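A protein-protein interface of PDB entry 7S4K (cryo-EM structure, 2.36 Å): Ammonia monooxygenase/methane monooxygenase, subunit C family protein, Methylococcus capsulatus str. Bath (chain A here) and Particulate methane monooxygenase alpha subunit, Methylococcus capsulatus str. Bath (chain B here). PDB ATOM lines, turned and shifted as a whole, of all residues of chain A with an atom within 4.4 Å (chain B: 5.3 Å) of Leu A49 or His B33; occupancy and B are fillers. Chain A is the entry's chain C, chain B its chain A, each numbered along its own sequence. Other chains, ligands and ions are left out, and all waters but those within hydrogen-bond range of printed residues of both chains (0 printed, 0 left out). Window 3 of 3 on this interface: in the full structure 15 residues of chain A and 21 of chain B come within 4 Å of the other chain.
The side-chain carboxylate of Asp A137 sits close to the backbone carbonyl oxygen of His B33 (2.9 Å).
OD1 of Asp A137 lies close to O of Gly B34.
OD1 of Asp A137 sits close to O of Glu B35.
Printed residues of chain B within 4 Å of Leu A49: His B33 (3.3 Å).
Printed residues of chain A within 4 Å of His B33: Leu A49 (3.3 Å) and Asp A137 (2.9 Å).
Printed residues of chain A within 4 Å of Gly B34: Asp A137 (3.1 Å).
Printed residues of chain B within 4 Å of Asp A137: His B33 (2.9 Å), Gly B34 (3.1 Å) and Glu B35 (3.1 Å).
The backbone NH (N) of His B33 sits at hydrogen-bond distance from the side-chain carboxylate (OE1) of Glu B35 (2.8 Å).
N of Ser A51 is in hydrogen-bond range of OD2 of Asp A137, at 3.3 Å.
The backbone carbonyl oxygen of Gly A44 lies within hydrogen-bond range of the backbone NH of Leu A49 (3.3 Å).
Pro B94 touches Trp A45 (CB to CD1, 3.5 Å).
Leu A49 touches His B33.
Hydrophobic or aromatic side chains of chain B within 4 Å of the printed part of chain A: His B33 and Pro B94.
Among the printed residues, 5 pairs touch across the chains.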
ATOM      1  N   GLY A  44     -18.228  -4.373   0.906  1.00  0.00           N
ATOM      2  CA  GLY A  44     -18.576  -5.673   1.445  1.00  0.00           C
ATOM      3  C   GLY A  44     -18.772  -6.676   0.331  1.00  0.00           C
ATOM      4  O   GLY A  44     -17.985  -7.612   0.180  1.00  0.00           O
ATOM      5  N   TRP A  45     -19.828  -6.492  -0.451  1.00  0.00           N
ATOM      6  CA  TRP A  45     -19.899  -7.105  -1.764  1.00  0.00           C
ATOM      7  C   TRP A  45     -19.088  -6.258  -2.730  1.00  0.00           C
ATOM      8  O   TRP A  45     -18.606  -5.181  -2.371  1.00  0.00           O
ATOM      9  CB  TRP A  45     -21.348  -7.220  -2.240  1.00  0.00           C
ATOM     10  CG  TRP A  45     -22.353  -7.297  -1.132  1.00  0.00           C
ATOM     11  CD1 TRP A  45     -23.022  -8.407  -0.707  1.00  0.00           C
ATOM     12  CD2 TRP A  45     -22.820  -6.215  -0.321  1.00  0.00           C
ATOM     13  NE1 TRP A  45     -23.866  -8.086   0.326  1.00  0.00           N
ATOM     14  CE2 TRP A  45     -23.760  -6.745   0.582  1.00  0.00           C
ATOM     15  CE3 TRP A  45     -22.526  -4.850  -0.265  1.00  0.00           C
ATOM     16  CZ2 TRP A  45     -24.408  -5.960   1.525  1.00  0.00           C
ATOM     17  CZ3 TRP A  45     -23.170  -4.074   0.671  1.00  0.00           C
ATOM     18  CH2 TRP A  45     -24.101  -4.629   1.553  1.00  0.00           C
ATOM     19  N   SER A  46     -18.944  -6.744  -3.966  1.00  0.00           N
ATOM     20  CA  SER A  46     -18.225  -5.964  -4.967  1.00  0.00           C
ATOM     21  C   SER A  46     -16.790  -5.699  -4.531  1.00  0.00           C
ATOM     22  O   SER A  46     -16.494  -4.599  -4.054  1.00  0.00           O
ATOM     23  CB  SER A  46     -18.938  -4.640  -5.256  1.00  0.00           C
ATOM     24  OG  SER A  46     -18.577  -3.659  -4.300  1.00  0.00           O
ATOM     25  N   ALA A  47     -15.912  -6.703  -4.654  1.00  0.00           N
ATOM     26  CA  ALA A  47     -14.556  -6.665  -4.096  1.00  0.00           C
ATOM     27  C   ALA A  47     -14.569  -6.767  -2.574  1.00  0.00           C
ATOM     28  O   ALA A  47     -14.394  -5.786  -1.852  1.00  0.00           O
ATOM     29  CB  ALA A  47     -13.784  -5.424  -4.554  1.00  0.00           C
ATOM     30  N   GLY A  48     -14.782  -7.993  -2.095  1.00  0.00           N
ATOM     31  CA  GLY A  48     -14.929  -8.280  -0.683  1.00  0.00           C
ATOM     32  C   GLY A  48     -15.762  -9.513  -0.402  1.00  0.00           C
ATOM     33  O   GLY A  48     -15.828  -9.970   0.742  1.00  0.00           O
ATOM     34  N   LEU A  49     -16.398 -10.073  -1.433  1.00  0.00           N
ATOM     35  CA  LEU A  49     -17.028 -11.383  -1.290  1.00  0.00           C
ATOM     36  C   LEU A  49     -16.044 -12.508  -1.595  1.00  0.00           C
ATOM     37  O   LEU A  49     -15.931 -13.474  -0.834  1.00  0.00           O
ATOM     38  CB  LEU A  49     -18.253 -11.489  -2.200  1.00  0.00           C
ATOM     39  CG  LEU A  49     -19.476 -10.665  -1.807  1.00  0.00           C
ATOM     40  CD1 LEU A  49     -20.467 -10.616  -2.956  1.00  0.00           C
ATOM     41  CD2 LEU A  49     -20.120 -11.236  -0.558  1.00  0.00           C
ATOM     42  N   ASP A  50     -15.331 -12.404  -2.714  1.00  0.00           N
ATOM     43  CA  ASP A  50     -14.381 -13.433  -3.118  1.00  0.00           C
ATOM     44  C   ASP A  50     -13.002 -13.084  -2.574  1.00  0.00           C
ATOM     45  O   ASP A  50     -12.444 -12.035  -2.908  1.00  0.00           O
ATOM     46  CB  ASP A  50     -14.352 -13.556  -4.639  1.00  0.00           C
ATOM     47  CG  ASP A  50     -13.435 -14.665  -5.125  1.00  0.00           C
ATOM     48  OD1 ASP A  50     -12.931 -15.446  -4.290  1.00  0.00           O
ATOM     49  OD2 ASP A  50     -13.232 -14.767  -6.352  1.00  0.00           O
ATOM     50  N   SER A  51     -12.449 -13.969  -1.747  1.00  0.00           N
ATOM     51  CA  SER A  51     -11.174 -13.716  -1.085  1.00  0.00           C
ATOM     52  C   SER A  51      -9.971 -14.002  -1.971  1.00  0.00           C
ATOM     53  O   SER A  51      -8.844 -13.696  -1.570  1.00  0.00           O
ATOM     54  CB  SER A  51     -11.074 -14.550   0.192  1.00  0.00           C
ATOM     55  OG  SER A  51     -10.289 -15.709  -0.017  1.00  0.00           O
ATOM     56  N   ILE A 134     -23.202 -15.201   4.525  1.00  0.00           N
ATOM     57  CA  ILE A 134     -22.297 -15.630   3.413  1.00  0.00           C
ATOM     58  C   ILE A 134     -21.438 -16.811   3.882  1.00  0.00           C
ATOM     59  O   ILE A 134     -21.204 -16.923   5.102  1.00  0.00           O
ATOM     60  CB  ILE A 134     -21.424 -14.463   2.898  1.00  0.00           C
ATOM     61  CG1 ILE A 134     -20.688 -13.738   4.028  1.00  0.00           C
ATOM     62  CG2 ILE A 134     -22.237 -13.496   2.048  1.00  0.00           C
ATOM     63  CD1 ILE A 134     -19.190 -13.942   4.012  1.00  0.00           C
ATOM     64  N   ASP A 137     -14.961 -17.741   3.784  1.00  0.00           N
ATOM     65  CA  ASP A 137     -13.976 -17.986   2.743  1.00  0.00           C
ATOM     66  C   ASP A 137     -12.544 -17.983   3.251  1.00  0.00           C
ATOM     67  O   ASP A 137     -11.668 -18.535   2.576  1.00  0.00           O
ATOM     68  CB  ASP A 137     -14.108 -16.940   1.625  1.00  0.00           C
ATOM     69  CG  ASP A 137     -14.002 -17.547   0.244  1.00  0.00           C
ATOM     70  OD1 ASP A 137     -14.143 -18.781   0.125  1.00  0.00           O
ATOM     71  OD2 ASP A 137     -13.771 -16.792  -0.723  1.00  0.00           O
ATOM     72  N   HIS B  33     -19.213 -18.340  -3.833  1.00  0.00           N
ATOM     73  CA  HIS B  33     -18.189 -17.292  -3.553  1.00  0.00           C
ATOM     74  C   HIS B  33     -17.419 -17.799  -2.340  1.00  0.00           C
ATOM     75  O   HIS B  33     -16.287 -17.338  -2.128  1.00  0.00           O
ATOM     76  CB  HIS B  33     -18.791 -15.883  -3.319  1.00  0.00           C
ATOM     77  CG  HIS B  33     -18.860 -14.978  -4.514  1.00  0.00           C
ATOM     78  ND1 HIS B  33     -19.201 -15.464  -5.754  1.00  0.00           N
ATOM     79  CD2 HIS B  33     -18.672 -13.635  -4.678  1.00  0.00           C
ATOM     80  CE1 HIS B  33     -19.186 -14.480  -6.630  1.00  0.00           C
ATOM     81  NE2 HIS B  33     -18.933 -13.351  -5.996  1.00  0.00           N
ATOM     82  N   GLY B  34     -18.024 -18.738  -1.601  1.00  0.00           N
ATOM     83  CA  GLY B  34     -17.369 -19.331  -0.419  1.00  0.00           C
ATOM     84  C   GLY B  34     -16.587 -20.584  -0.768  1.00  0.00           C
ATOM     85  O   GLY B  34     -16.021 -21.191   0.158  1.00  0.00           O
ATOM     86  N   GLU B  35     -16.556 -20.968  -2.048  1.00  0.00           N
ATOM     87  CA  GLU B  35     -15.722 -22.122  -2.489  1.00  0.00           C
ATOM     88  C   GLU B  35     -14.342 -21.583  -2.902  1.00  0.00           C
ATOM     89  O   GLU B  35     -14.002 -20.465  -2.445  1.00  0.00           O
ATOM     90  CB  GLU B  35     -16.449 -22.936  -3.568  1.00  0.00           C
ATOM     91  CG  GLU B  35     -16.579 -22.258  -4.924  1.00  0.00           C
ATOM     92  CD  GLU B  35     -17.440 -21.008  -4.988  1.00  0.00           C
ATOM     93  OE1 GLU B  35     -18.470 -20.960  -4.289  1.00  0.00           O
ATOM     94  OE2 GLU B  35     -17.066 -20.083  -5.721  1.00  0.00           O
ATOM     95  N   PRO B  94     -25.636 -13.551  -1.666  1.00  0.00           N
ATOM     96  CA  PRO B  94     -25.242 -12.549  -0.666  1.00  0.00           C
ATOM     97  C   PRO B  94     -26.436 -11.986   0.085  1.00  0.00           C
ATOM     98  O   PRO B  94     -26.848 -10.849  -0.161  1.00  0.00           O
ATOM     99  CB  PRO B  94     -24.550 -11.462  -1.500  1.00  0.00           C
ATOM    100  CG  PRO B  94     -24.497 -11.982  -2.907  1.00  0.00           C
ATOM    101  CD  PRO B  94     -25.552 -13.017  -3.032  1.00  0.00           C
ATOM    102  N   HIS B 137     -24.263 -13.628  -7.677  1.00  0.00           N
ATOM    103  CA  HIS B 137     -23.728 -14.947  -7.990  1.00  0.00           C
ATOM    104  C   HIS B 137     -24.520 -15.960  -7.174  1.00  0.00           C
ATOM    105  O   HIS B 137     -24.256 -16.160  -5.987  1.00  0.00           O
ATOM    106  CB  HIS B 137     -22.240 -15.009  -7.678  1.00  0.00           C
ATOM    107  CG  HIS B 137     -21.478 -15.952  -8.551  1.00  0.00           C
ATOM    108  ND1 HIS B 137     -20.561 -16.852  -8.053  1.00  0.00           N
ATOM    109  CD2 HIS B 137     -21.494 -16.136  -9.893  1.00  0.00           C
ATOM    110  CE1 HIS B 137     -20.046 -17.549  -9.049  1.00  0.00           C
ATOM    111  NE2 HIS B 137     -20.595 -17.134 -10.175  1.00  0.00           N
ATOM    112  N   HIS B 139     -25.597 -19.550  -6.092  1.00  0.00           N
ATOM    113  CA  HIS B 139     -25.134 -20.924  -6.020  1.00  0.00           C
ATOM    114  C   HIS B 139     -26.254 -21.811  -5.503  1.00  0.00           C
ATOM    115  O   HIS B 139     -27.101 -21.376  -4.719  1.00  0.00           O
ATOM    116  CB  HIS B 139     -23.927 -21.073  -5.090  1.00  0.00           C
ATOM    117  CG  HIS B 139     -22.691 -20.391  -5.579  1.00  0.00           C
ATOM    118  ND1 HIS B 139     -21.620 -21.080  -6.103  1.00  0.00           N
ATOM    119  CD2 HIS B 139     -22.345 -19.083  -5.603  1.00  0.00           C
ATOM    120  CE1 HIS B 139     -20.672 -20.226  -6.440  1.00  0.00           C
ATOM    121  NE2 HIS B 139     -21.086 -19.007  -6.146  1.00  0.00           N
ATOM    122  N   ILE B 151     -20.992 -26.394  -1.809  1.00  0.00           N
ATOM    123  CA  ILE B 151     -21.424 -25.364  -2.743  1.00  0.00           C
ATOM    124  C   ILE B 151     -21.320 -25.884  -4.168  1.00  0.00           C
ATOM    125  O   ILE B 151     -20.267 -26.373  -4.596  1.00  0.00           O
ATOM    126  CB  ILE B 151     -20.594 -24.088  -2.555  1.00  0.00           C
ATOM    127  CG1 ILE B 151     -20.648 -23.632  -1.097  1.00  0.00           C
ATOM    128  CG2 ILE B 151     -21.087 -22.993  -3.470  1.00  0.00           C
ATOM    129  CD1 ILE B 151     -19.300 -23.534  -0.442  1.00  0.00           C
ATOM    130  N   TRP B 156     -24.121 -15.983 -12.503  1.00  0.00           N
ATOM    131  CA  TRP B 156     -24.441 -14.573 -12.339  1.00  0.00           C
ATOM    132  C   TRP B 156     -25.848 -14.294 -12.843  1.00  0.00           C
ATOM    133  O   TRP B 156     -26.150 -14.498 -14.022  1.00  0.00           O
ATOM    134  CB  TRP B 156     -23.433 -13.706 -13.089  1.00  0.00           C
ATOM    135  CG  TRP B 156     -22.092 -13.667 -12.448  1.00  0.00           C
ATOM    136  CD1 TRP B 156     -20.976 -14.333 -12.846  1.00  0.00           C
ATOM    137  CD2 TRP B 156     -21.723 -12.924 -11.282  1.00  0.00           C
ATOM    138  NE1 TRP B 156     -19.930 -14.052 -12.004  1.00  0.00           N
ATOM    139  CE2 TRP B 156     -20.364 -13.189 -11.034  1.00  0.00           C
ATOM    140  CE3 TRP B 156     -22.410 -12.062 -10.425  1.00  0.00           C
ATOM    141  CZ2 TRP B 156     -19.679 -12.622  -9.966  1.00  0.00           C
ATOM    142  CZ3 TRP B 156     -21.728 -11.501  -9.366  1.00  0.00           C
ATOM    143  CH2 TRP B 156     -20.377 -11.783  -9.145  1.00  0.00           C
